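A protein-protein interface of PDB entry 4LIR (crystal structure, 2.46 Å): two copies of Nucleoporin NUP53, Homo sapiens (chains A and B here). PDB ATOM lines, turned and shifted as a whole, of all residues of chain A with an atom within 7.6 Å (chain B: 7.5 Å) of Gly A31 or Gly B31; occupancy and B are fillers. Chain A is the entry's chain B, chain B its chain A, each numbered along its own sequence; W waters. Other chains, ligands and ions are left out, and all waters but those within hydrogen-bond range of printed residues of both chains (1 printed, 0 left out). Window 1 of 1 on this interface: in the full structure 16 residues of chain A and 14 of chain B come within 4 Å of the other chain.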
ATOM      1  N   VAL A  29      17.204  35.549 -22.888  1.00  0.00           N
ATOM      2  CA  VAL A  29      17.278  34.310 -22.101  1.00  0.00           C
ATOM      3  C   VAL A  29      16.592  33.237 -22.934  1.00  0.00           C
ATOM      4  O   VAL A  29      15.509  33.482 -23.476  1.00  0.00           O
ATOM      5  CB  VAL A  29      16.677  34.487 -20.687  1.00  0.00           C
ATOM      6  CG1 VAL A  29      16.659  33.176 -19.923  1.00  0.00           C
ATOM      7  CG2 VAL A  29      17.449  35.549 -19.906  1.00  0.00           C
ATOM      8  N   PHE A  30      17.247  32.074 -23.109  1.00  0.00           N
ATOM      9  CA  PHE A  30      16.689  31.060 -24.009  1.00  0.00           C
ATOM     10  C   PHE A  30      16.989  29.631 -23.585  1.00  0.00           C
ATOM     11  O   PHE A  30      17.810  29.407 -22.697  1.00  0.00           O
ATOM     12  CB  PHE A  30      17.225  31.299 -25.427  1.00  0.00           C
ATOM     13  CG  PHE A  30      18.727  31.238 -25.614  1.00  0.00           C
ATOM     14  CD1 PHE A  30      19.513  32.376 -25.450  1.00  0.00           C
ATOM     15  CD2 PHE A  30      19.351  30.059 -26.034  1.00  0.00           C
ATOM     16  CE1 PHE A  30      20.883  32.340 -25.725  1.00  0.00           C
ATOM     17  CE2 PHE A  30      20.726  30.017 -26.263  1.00  0.00           C
ATOM     18  CZ  PHE A  30      21.480  31.155 -26.112  1.00  0.00           C
ATOM     19  N   GLY A  31      16.325  28.690 -24.258  1.00  0.00           N
ATOM     20  CA  GLY A  31      16.512  27.255 -24.079  1.00  0.00           C
ATOM     21  C   GLY A  31      15.581  26.541 -23.132  1.00  0.00           C
ATOM     22  O   GLY A  31      15.861  25.405 -22.754  1.00  0.00           O
ATOM     23  N   PHE A  32      14.480  27.176 -22.725  1.00  0.00           N
ATOM     24  CA  PHE A  32      13.571  26.577 -21.748  1.00  0.00           C
ATOM     25  C   PHE A  32      12.304  25.997 -22.396  1.00  0.00           C
ATOM     26  O   PHE A  32      11.799  26.599 -23.351  1.00  0.00           O
ATOM     27  CB  PHE A  32      13.187  27.640 -20.684  1.00  0.00           C
ATOM     28  CG  PHE A  32      12.775  28.962 -21.294  1.00  0.00           C
ATOM     29  CD1 PHE A  32      13.710  29.973 -21.507  1.00  0.00           C
ATOM     30  CD2 PHE A  32      11.448  29.197 -21.660  1.00  0.00           C
ATOM     31  CE1 PHE A  32      13.328  31.186 -22.096  1.00  0.00           C
ATOM     32  CE2 PHE A  32      11.083  30.382 -22.299  1.00  0.00           C
ATOM     33  CZ  PHE A  32      12.019  31.371 -22.502  1.00  0.00           C
ATOM     34  N   PRO A  33      11.739  24.877 -21.864  1.00  0.00           N
ATOM     35  CA  PRO A  33      10.433  24.393 -22.366  1.00  0.00           C
ATOM     36  C   PRO A  33       9.326  25.409 -22.032  1.00  0.00           C
ATOM     37  O   PRO A  33       9.522  26.209 -21.099  1.00  0.00           O
ATOM     38  CB  PRO A  33      10.224  23.071 -21.605  1.00  0.00           C
ATOM     39  CG  PRO A  33      11.042  23.169 -20.414  1.00  0.00           C
ATOM     40  CD  PRO A  33      12.194  24.081 -20.703  1.00  0.00           C
ATOM     41  N   GLN A  34       8.181  25.397 -22.771  1.00  0.00           N
ATOM     42  CA  GLN A  34       7.131  26.408 -22.581  1.00  0.00           C
ATOM     43  C   GLN A  34       6.604  26.465 -21.125  1.00  0.00           C
ATOM     44  O   GLN A  34       6.421  27.559 -20.596  1.00  0.00           O
ATOM     45  CB  GLN A  34       5.973  26.243 -23.597  1.00  0.00           C
ATOM     46  CG  GLN A  34       4.878  25.232 -23.218  1.00  0.00           C
ATOM     47  CD  GLN A  34       3.664  25.856 -22.526  1.00  0.00           C
ATOM     48  OE1 GLN A  34       3.283  27.017 -22.774  1.00  0.00           O
ATOM     49  NE2 GLN A  34       3.013  25.081 -21.652  1.00  0.00           N
ATOM     50  N   ILE A  40      11.694  30.527 -15.173  1.00  0.00           N
ATOM     51  CA  ILE A  40      12.918  31.145 -15.668  1.00  0.00           C
ATOM     52  C   ILE A  40      12.859  32.691 -15.498  1.00  0.00           C
ATOM     53  O   ILE A  40      13.847  33.278 -15.039  1.00  0.00           O
ATOM     54  CB  ILE A  40      13.232  30.695 -17.136  1.00  0.00           C
ATOM     55  CG1 ILE A  40      13.546  29.176 -17.219  1.00  0.00           C
ATOM     56  CG2 ILE A  40      14.363  31.519 -17.769  1.00  0.00           C
ATOM     57  CD1 ILE A  40      14.633  28.638 -16.261  1.00  0.00           C
ATOM     58  N   GLY A  59       9.017  31.135 -30.268  1.00  0.00           N
ATOM     59  CA  GLY A  59      10.137  30.267 -29.902  1.00  0.00           C
ATOM     60  C   GLY A  59      10.485  30.256 -28.440  1.00  0.00           C
ATOM     61  O   GLY A  59       9.852  30.962 -27.665  1.00  0.00           O
ATOM     62  N   ASN A  60      11.521  29.483 -28.058  1.00  0.00           N
ATOM     63  CA  ASN A  60      11.922  29.219 -26.666  1.00  0.00           C
ATOM     64  C   ASN A  60      12.852  30.298 -26.064  1.00  0.00           C
ATOM     65  O   ASN A  60      13.866  29.964 -25.433  1.00  0.00           O
ATOM     66  CB  ASN A  60      12.590  27.834 -26.583  1.00  0.00           C
ATOM     67  CG  ASN A  60      13.865  27.731 -27.372  1.00  0.00           C
ATOM     68  OD1 ASN A  60      14.162  28.520 -28.272  1.00  0.00           O
ATOM     69  ND2 ASN A  60      14.694  26.820 -26.958  1.00  0.00           N
ATOM     70  N   TRP A  61      12.473  31.587 -26.209  1.00  0.00           N
ATOM     71  CA  TRP A  61      13.284  32.661 -25.656  1.00  0.00           C
ATOM     72  C   TRP A  61      12.450  33.811 -25.171  1.00  0.00           C
ATOM     73  O   TRP A  61      11.282  33.948 -25.513  1.00  0.00           O
ATOM     74  CB  TRP A  61      14.354  33.175 -26.659  1.00  0.00           C
ATOM     75  CG  TRP A  61      13.818  33.794 -27.920  1.00  0.00           C
ATOM     76  CD1 TRP A  61      13.535  35.120 -28.129  1.00  0.00           C
ATOM     77  CD2 TRP A  61      13.490  33.112 -29.144  1.00  0.00           C
ATOM     78  NE1 TRP A  61      13.071  35.309 -29.416  1.00  0.00           N
ATOM     79  CE2 TRP A  61      13.035  34.094 -30.063  1.00  0.00           C
ATOM     80  CE3 TRP A  61      13.544  31.766 -29.558  1.00  0.00           C
ATOM     81  CZ2 TRP A  61      12.628  33.772 -31.366  1.00  0.00           C
ATOM     82  CZ3 TRP A  61      13.131  31.443 -30.843  1.00  0.00           C
ATOM     83  CH2 TRP A  61      12.674  32.438 -31.730  1.00  0.00           C
ATOM     84  N   MET A  62      13.083  34.652 -24.357  1.00  0.00           N
ATOM     85  CA  MET A  62      12.513  35.853 -23.812  1.00  0.00           C
ATOM     86  C   MET A  62      13.569  36.970 -23.795  1.00  0.00           C
ATOM     87  O   MET A  62      14.756  36.703 -23.596  1.00  0.00           O
ATOM     88  CB  MET A  62      11.925  35.612 -22.427  1.00  0.00           C
ATOM     89  CG  MET A  62      12.963  35.301 -21.359  1.00  0.00           C
ATOM     90  SD  MET A  62      12.150  35.143 -19.624  1.00  0.00           S
ATOM     91  CE  MET A  62      11.530  33.359 -19.733  1.00  0.00           C
ATOM     92  N   SER A  86      17.673  20.362 -14.797  1.00  0.00           N
ATOM     93  CA  SER A  86      17.235  19.867 -16.109  1.00  0.00           C
ATOM     94  C   SER A  86      17.245  20.921 -17.228  1.00  0.00           C
ATOM     95  O   SER A  86      17.104  20.550 -18.394  1.00  0.00           O
ATOM     96  CB  SER A  86      15.823  19.303 -15.999  1.00  0.00           C
ATOM     97  OG  SER A  86      14.915  20.322 -15.608  1.00  0.00           O
ATOM     98  N   ILE A  87      17.320  22.219 -16.889  1.00  0.00           N
ATOM     99  CA  ILE A  87      17.271  23.248 -17.912  1.00  0.00           C
ATOM    100  C   ILE A  87      18.581  24.024 -17.948  1.00  0.00           C
ATOM    101  O   ILE A  87      18.848  24.855 -17.084  1.00  0.00           O
ATOM    102  CB  ILE A  87      16.044  24.216 -17.774  1.00  0.00           C
ATOM    103  CG1 ILE A  87      14.698  23.469 -17.614  1.00  0.00           C
ATOM    104  CG2 ILE A  87      15.985  25.206 -18.939  1.00  0.00           C
ATOM    105  CD1 ILE A  87      13.604  24.294 -16.771  1.00  0.00           C
ATOM    106  N   MET A  88      19.389  23.754 -18.974  1.00  0.00           N
ATOM    107  CA  MET A  88      20.575  24.545 -19.263  1.00  0.00           C
ATOM    108  C   MET A  88      20.043  25.754 -20.042  1.00  0.00           C
ATOM    109  O   MET A  88      19.339  25.584 -21.045  1.00  0.00           O
ATOM    110  CB  MET A  88      21.634  23.748 -20.045  1.00  0.00           C
ATOM    111  CG  MET A  88      22.978  24.458 -20.079  1.00  0.00           C
ATOM    112  SD  MET A  88      24.330  23.463 -20.965  1.00  0.00           S
ATOM    113  CE  MET A  88      24.556  22.108 -19.697  1.00  0.00           C
ATOM    114  N   ILE A  89      20.287  26.947 -19.513  1.00  0.00           N
ATOM    115  CA  ILE A  89      19.795  28.211 -20.039  1.00  0.00           C
ATOM    116  C   ILE A  89      20.918  28.956 -20.756  1.00  0.00           C
ATOM    117  O   ILE A  89      22.076  28.960 -20.322  1.00  0.00           O
ATOM    118  CB  ILE A  89      19.197  29.040 -18.846  1.00  0.00           C
ATOM    119  CG1 ILE A  89      17.817  28.495 -18.377  1.00  0.00           C
ATOM    120  CG2 ILE A  89      19.148  30.545 -19.112  1.00  0.00           C
ATOM    121  CD1 ILE A  89      16.604  28.752 -19.336  1.00  0.00           C
ATOM    122  N   GLY A  90      20.543  29.561 -21.868  1.00  0.00           N
ATOM    123  CA  GLY A  90      21.405  30.424 -22.646  1.00  0.00           C
ATOM    124  C   GLY A  90      21.072  31.863 -22.321  1.00  0.00           C
ATOM    125  O   GLY A  90      19.899  32.191 -22.075  1.00  0.00           O
ATOM    126  N   VAL A  91      22.107  32.719 -22.269  1.00  0.00           N
ATOM    127  CA  VAL A  91      21.969  34.160 -22.003  1.00  0.00           C
ATOM    128  C   VAL A  91      22.915  34.907 -22.934  1.00  0.00           C
ATOM    129  O   VAL A  91      24.136  34.730 -22.868  1.00  0.00           O
ATOM    130  CB  VAL A  91      22.161  34.626 -20.528  1.00  0.00           C
ATOM    131  CG1 VAL A  91      21.580  36.032 -20.333  1.00  0.00           C
ATOM    132  CG2 VAL A  91      21.535  33.655 -19.536  1.00  0.00           C
ATOM    133  N   VAL B  29      25.872  21.384 -26.843  1.00  0.00           N
ATOM    134  CA  VAL B  29      24.744  21.999 -27.560  1.00  0.00           C
ATOM    135  C   VAL B  29      23.558  21.920 -26.621  1.00  0.00           C
ATOM    136  O   VAL B  29      23.329  20.867 -26.028  1.00  0.00           O
ATOM    137  CB  VAL B  29      24.499  21.323 -28.933  1.00  0.00           C
ATOM    138  CG1 VAL B  29      23.250  21.875 -29.612  1.00  0.00           C
ATOM    139  CG2 VAL B  29      25.718  21.493 -29.833  1.00  0.00           C
ATOM    140  N   PHE B  30      22.844  23.030 -26.424  1.00  0.00           N
ATOM    141  CA  PHE B  30      21.753  23.027 -25.449  1.00  0.00           C
ATOM    142  C   PHE B  30      20.591  23.948 -25.834  1.00  0.00           C
ATOM    143  O   PHE B  30      20.712  24.764 -26.744  1.00  0.00           O
ATOM    144  CB  PHE B  30      22.300  23.423 -24.059  1.00  0.00           C
ATOM    145  CG  PHE B  30      22.941  24.789 -23.943  1.00  0.00           C
ATOM    146  CD1 PHE B  30      24.298  24.965 -24.214  1.00  0.00           C
ATOM    147  CD2 PHE B  30      22.206  25.887 -23.502  1.00  0.00           C
ATOM    148  CE1 PHE B  30      24.908  26.218 -24.044  1.00  0.00           C
ATOM    149  CE2 PHE B  30      22.807  27.145 -23.359  1.00  0.00           C
ATOM    150  CZ  PHE B  30      24.156  27.300 -23.622  1.00  0.00           C
ATOM    151  N   GLY B  31      19.494  23.815 -25.100  1.00  0.00           N
ATOM    152  CA  GLY B  31      18.297  24.627 -25.267  1.00  0.00           C
ATOM    153  C   GLY B  31      17.228  24.021 -26.148  1.00  0.00           C
ATOM    154  O   GLY B  31      16.318  24.712 -26.587  1.00  0.00           O
ATOM    155  N   PHE B  32      17.296  22.731 -26.386  1.00  0.00           N
ATOM    156  CA  PHE B  32      16.295  22.099 -27.221  1.00  0.00           C
ATOM    157  C   PHE B  32      15.414  21.140 -26.433  1.00  0.00           C
ATOM    158  O   PHE B  32      15.925  20.433 -25.555  1.00  0.00           O
ATOM    159  CB  PHE B  32      16.973  21.338 -28.371  1.00  0.00           C
ATOM    160  CG  PHE B  32      18.056  20.389 -27.917  1.00  0.00           C
ATOM    161  CD1 PHE B  32      19.369  20.828 -27.766  1.00  0.00           C
ATOM    162  CD2 PHE B  32      17.764  19.056 -27.634  1.00  0.00           C
ATOM    163  CE1 PHE B  32      20.360  19.966 -27.316  1.00  0.00           C
ATOM    164  CE2 PHE B  32      18.759  18.192 -27.181  1.00  0.00           C
ATOM    165  CZ  PHE B  32      20.049  18.651 -27.029  1.00  0.00           C
ATOM    166  N   PRO B  33      14.113  21.009 -26.796  1.00  0.00           N
ATOM    167  CA  PRO B  33      13.279  19.956 -26.163  1.00  0.00           C
ATOM    168  C   PRO B  33      13.704  18.555 -26.651  1.00  0.00           C
ATOM    169  O   PRO B  33      14.302  18.444 -27.720  1.00  0.00           O
ATOM    170  CB  PRO B  33      11.863  20.318 -26.601  1.00  0.00           C
ATOM    171  CG  PRO B  33      12.024  21.083 -27.866  1.00  0.00           C
ATOM    172  CD  PRO B  33      13.374  21.746 -27.845  1.00  0.00           C
ATOM    173  N   SER B  36      13.065  17.251 -30.211  1.00  0.00           N
ATOM    174  CA  SER B  36      13.889  17.928 -31.222  1.00  0.00           C
ATOM    175  C   SER B  36      15.350  17.477 -31.245  1.00  0.00           C
ATOM    176  O   SER B  36      16.120  18.006 -32.045  1.00  0.00           O
ATOM    177  CB  SER B  36      13.856  19.428 -30.980  1.00  0.00           C
ATOM    178  OG  SER B  36      12.538  19.896 -31.176  1.00  0.00           O
ATOM    179  N   ILE B  40      18.250  18.529 -34.021  1.00  0.00           N
ATOM    180  CA  ILE B  40      19.401  19.336 -33.614  1.00  0.00           C
ATOM    181  C   ILE B  40      20.727  18.589 -33.917  1.00  0.00           C
ATOM    182  O   ILE B  40      21.647  19.211 -34.448  1.00  0.00           O
ATOM    183  CB  ILE B  40      19.281  19.794 -32.120  1.00  0.00           C
ATOM    184  CG1 ILE B  40      18.100  20.782 -31.930  1.00  0.00           C
ATOM    185  CG2 ILE B  40      20.591  20.433 -31.598  1.00  0.00           C
ATOM    186  CD1 ILE B  40      18.076  22.067 -32.928  1.00  0.00           C
ATOM    187  N   GLY B  59      18.495  16.308 -18.915  1.00  0.00           N
ATOM    188  CA  GLY B  59      18.557  17.673 -19.413  1.00  0.00           C
ATOM    189  C   GLY B  59      18.357  17.957 -20.882  1.00  0.00           C
ATOM    190  O   GLY B  59      18.385  17.058 -21.729  1.00  0.00           O
ATOM    191  N   ASN B  60      18.226  19.252 -21.188  1.00  0.00           N
ATOM    192  CA  ASN B  60      18.063  19.741 -22.548  1.00  0.00           C
ATOM    193  C   ASN B  60      19.426  20.026 -23.237  1.00  0.00           C
ATOM    194  O   ASN B  60      19.575  21.051 -23.900  1.00  0.00           O
ATOM    195  CB  ASN B  60      17.178  20.979 -22.542  1.00  0.00           C
ATOM    196  CG  ASN B  60      17.750  22.169 -21.833  1.00  0.00           C
ATOM    197  OD1 ASN B  60      18.631  22.057 -20.986  1.00  0.00           O
ATOM    198  ND2 ASN B  60      17.321  23.343 -22.228  1.00  0.00           N
ATOM    199  N   TRP B  61      20.405  19.106 -23.116  1.00  0.00           N
ATOM    200  CA  TRP B  61      21.706  19.305 -23.756  1.00  0.00           C
ATOM    201  C   TRP B  61      22.305  18.008 -24.246  1.00  0.00           C
ATOM    202  O   TRP B  61      21.867  16.917 -23.866  1.00  0.00           O
ATOM    203  CB  TRP B  61      22.716  20.017 -22.821  1.00  0.00           C
ATOM    204  CG  TRP B  61      23.072  19.274 -21.565  1.00  0.00           C
ATOM    205  CD1 TRP B  61      24.109  18.402 -21.388  1.00  0.00           C
ATOM    206  CD2 TRP B  61      22.394  19.352 -20.306  1.00  0.00           C
ATOM    207  NE1 TRP B  61      24.118  17.933 -20.093  1.00  0.00           N
ATOM    208  CE2 TRP B  61      23.073  18.495 -19.407  1.00  0.00           C
ATOM    209  CE3 TRP B  61      21.286  20.083 -19.838  1.00  0.00           C
ATOM    210  CZ2 TRP B  61      22.671  18.340 -18.076  1.00  0.00           C
ATOM    211  CZ3 TRP B  61      20.890  19.928 -18.521  1.00  0.00           C
ATOM    212  CH2 TRP B  61      21.575  19.065 -17.653  1.00  0.00           C
ATOM    213  N   MET B  62      23.326  18.142 -25.092  1.00  0.00           N
ATOM    214  CA  MET B  62      24.105  17.030 -25.613  1.00  0.00           C
ATOM    215  C   MET B  62      25.545  17.455 -25.808  1.00  0.00           C
ATOM    216  O   MET B  62      25.849  18.641 -25.998  1.00  0.00           O
ATOM    217  CB  MET B  62      23.527  16.449 -26.922  1.00  0.00           C
ATOM    218  CG  MET B  62      23.601  17.385 -28.108  1.00  0.00           C
ATOM    219  SD  MET B  62      22.964  16.598 -29.756  1.00  0.00           S
ATOM    220  CE  MET B  62      21.157  16.474 -29.488  1.00  0.00           C
ATOM    221  N   SER B  86      12.007  28.523 -34.271  1.00  0.00           N
ATOM    222  CA  SER B  86      11.438  28.276 -32.940  1.00  0.00           C
ATOM    223  C   SER B  86      12.448  27.856 -31.877  1.00  0.00           C
ATOM    224  O   SER B  86      12.122  27.922 -30.694  1.00  0.00           O
ATOM    225  CB  SER B  86      10.353  27.207 -33.036  1.00  0.00           C
ATOM    226  OG  SER B  86      10.892  25.976 -33.497  1.00  0.00           O
ATOM    227  N   ILE B  87      13.627  27.373 -32.269  1.00  0.00           N
ATOM    228  CA  ILE B  87      14.587  26.909 -31.273  1.00  0.00           C
ATOM    229  C   ILE B  87      15.863  27.734 -31.299  1.00  0.00           C
ATOM    230  O   ILE B  87      16.661  27.610 -32.220  1.00  0.00           O
ATOM    231  CB  ILE B  87      14.916  25.376 -31.410  1.00  0.00           C
ATOM    232  CG1 ILE B  87      13.642  24.509 -31.418  1.00  0.00           C
ATOM    233  CG2 ILE B  87      15.836  24.915 -30.256  1.00  0.00           C
ATOM    234  CD1 ILE B  87      13.863  23.057 -31.870  1.00  0.00           C
ATOM    235  N   MET B  88      16.050  28.575 -30.283  1.00  0.00           N
ATOM    236  CA  MET B  88      17.289  29.296 -30.082  1.00  0.00           C
ATOM    237  C   MET B  88      18.187  28.320 -29.353  1.00  0.00           C
ATOM    238  O   MET B  88      17.802  27.787 -28.300  1.00  0.00           O
ATOM    239  CB  MET B  88      17.092  30.623 -29.296  1.00  0.00           C
ATOM    240  CG  MET B  88      18.349  31.514 -29.339  1.00  0.00           C
ATOM    241  SD  MET B  88      18.123  33.207 -28.488  1.00  0.00           S
ATOM    242  CE  MET B  88      16.951  33.947 -29.698  1.00  0.00           C
ATOM    243  N   ILE B  89      19.353  28.036 -29.943  1.00  0.00           N
ATOM    244  CA  ILE B  89      20.294  27.040 -29.442  1.00  0.00           C
ATOM    245  C   ILE B  89      21.549  27.679 -28.826  1.00  0.00           C
ATOM    246  O   ILE B  89      22.124  28.622 -29.382  1.00  0.00           O
ATOM    247  CB  ILE B  89      20.640  26.109 -30.657  1.00  0.00           C
ATOM    248  CG1 ILE B  89      19.542  25.030 -30.869  1.00  0.00           C
ATOM    249  CG2 ILE B  89      22.062  25.486 -30.611  1.00  0.00           C
ATOM    250  CD1 ILE B  89      19.352  23.987 -29.722  1.00  0.00           C
ATOM    251  N   GLY B  90      21.974  27.105 -27.707  1.00  0.00           N
ATOM    252  CA  GLY B  90      23.201  27.473 -27.024  1.00  0.00           C
ATOM    253  C   GLY B  90      24.300  26.507 -27.413  1.00  0.00           C
ATOM    254  O   GLY B  90      24.042  25.309 -27.607  1.00  0.00           O
ATOM    255  N   VAL B  91      25.527  27.032 -27.591  1.00  0.00           N
ATOM    256  CA  VAL B  91      26.712  26.238 -27.927  1.00  0.00           C
ATOM    257  C   VAL B  91      27.879  26.765 -27.115  1.00  0.00           C
ATOM    258  O   VAL B  91      28.277  27.929 -27.257  1.00  0.00           O
ATOM    259  CB  VAL B  91      27.081  26.153 -29.435  1.00  0.00           C
ATOM    260  CG1 VAL B  91      28.051  24.999 -29.676  1.00  0.00           C
ATOM    261  CG2 VAL B  91      25.843  26.021 -30.345  1.00  0.00           C
HETATM  262  O   HOH W   1      14.499  23.284 -24.054  1.00  0.00           O
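Phe A30 touches Met B88, and with the chains exchanged Met A88 touches Phe B30. Phe A30 touches Ile B89, and with the chains exchanged Ile A89 touches Phe B30. Gly A59 touches Ser B86, and with the chains exchanged Ser A86 touches Gly B59. Asn A60 touches Ser B86, and with the chains exchanged Ser A86 touches Asn B60. Of the 21 pairs that touch across the chains among the printed residues, 21 have their exchanged pair printed and touching as well.
CD1 of Phe A30 touches SD of Met B88, at 3.4 Å. CA of Gly B31 touches CA of Gly A31, 3.4 Å away. Gly A59 touches Ser B86 (CA to O, 3.2 Å). Asn A60 touches Ile B87. Trp A61 touches Ser B86 (CZ3 to O, 3.7 Å). CE of Met B88 touches CD2 of Trp A61, at 3.6 Å. O of Ser A86 touches CA of Gly B59 (3.4 Å). Ser A86 touches Trp B61. Phe B30 touches Met A88. Met A88 touches Trp B61.
Of the 17 printed residues of chain B, 10 touch a printed residue of chain A. Hydrophobic or aromatic side chains of chain B that line the printed part of chain A: Phe B30, Trp B61, Ile B87 and Met B88. Of the 17 printed residues of chain A, 10 touch a printed residue of chain B. Hydrophobic or aromatic side chains of chain A within 4 Å of the printed part of chain B: Phe A30, Trp A61 and Met A88. Among the printed residues, 21 pairs touch across the chains. Among the printed residues, no Asp or Glu carboxylate lies within 4 Å of a Lys or Arg side-chain nitrogen of the other chain.
Gly A31 touches just these residues of chain B: Gly B31 (3.4 Å) and Asn B60 (2.6 Å). Of the printed residues of chain B, Trp A61 touches Ser B86 (3.7 Å) and Met B88 (3.6 Å). Met A62 touches none of the printed residues of chain B. Of the printed residues of chain B, Gly A90 touches Phe B30 (3.6 Å). Gly B31 touches two residues of chain A. Printed residues of chain A within 4 Å of Trp B61: Ser A86 and Met A88. Of the printed residues of chain A, Met B88 touches Phe A30, Asn A60 and Trp A61. Printed residues of chain A within 4 Å of Gly B90: Phe A30 (3.5 Å). The nearest residue of chain B that does not touch Gly A31 is Met B88 (4.4 Å). The nearest residue of chain A that does not touch Gly B31 is Met A88 (4.4 Å).
The backbone NH (N) of Gly B31 lies within hydrogen-bond range of the backbone carbonyl oxygen (O) of Asn B60 (3.0 Å). The backbone carbonyl oxygen (O) of Gly A90 sits at hydrogen-bond distance from the backbone NH (N) of Phe A30 (2.8 Å). N of Gly B90 sits at hydrogen-bond distance from O of Phe B30 (2.8 Å). The backbone NH (N) of Gly A31 sits at hydrogen-bond distance from the backbone carbonyl oxygen (O) of Asn A60, at 3.0 Å.
Water W1 lies within hydrogen-bond range of the backbone carbonyl oxygen (O) of Gly A31 (2.8 Å), the side-chain amide nitrogen (ND2) of Asn B60 (3.4 Å) and the backbone carbonyl oxygen (O) of Gly B31 (3.4 Å).
The backbone carbonyl oxygen of Ser B86 sits at hydrogen-bond distance from the backbone NH of Asn A60 (3.1 Å). The side-chain amide nitrogen (ND2) of Asn B60 lies within hydrogen-bond range of the backbone carbonyl oxygen (O) of Gly A31 (2.6 Å). The side-chain amide oxygen (OD1) of Asn B60 sits at hydrogen-bond distance from the backbone NH (N) of Met A88 (2.7 Å). The backbone NH (N) of Asn B60 sits at hydrogen-bond distance from the backbone carbonyl oxygen (O) of Ser A86 (3.3 Å). The side-chain amide oxygen (OD1) of Asn A60 sits at hydrogen-bond distance from the backbone NH (N) of Met B88 (2.8 Å). The side-chain amide nitrogen (ND2) of Asn A60 sits at hydrogen-bond distance from the backbone carbonyl oxygen (O) of Gly B31, at 2.7 Å.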
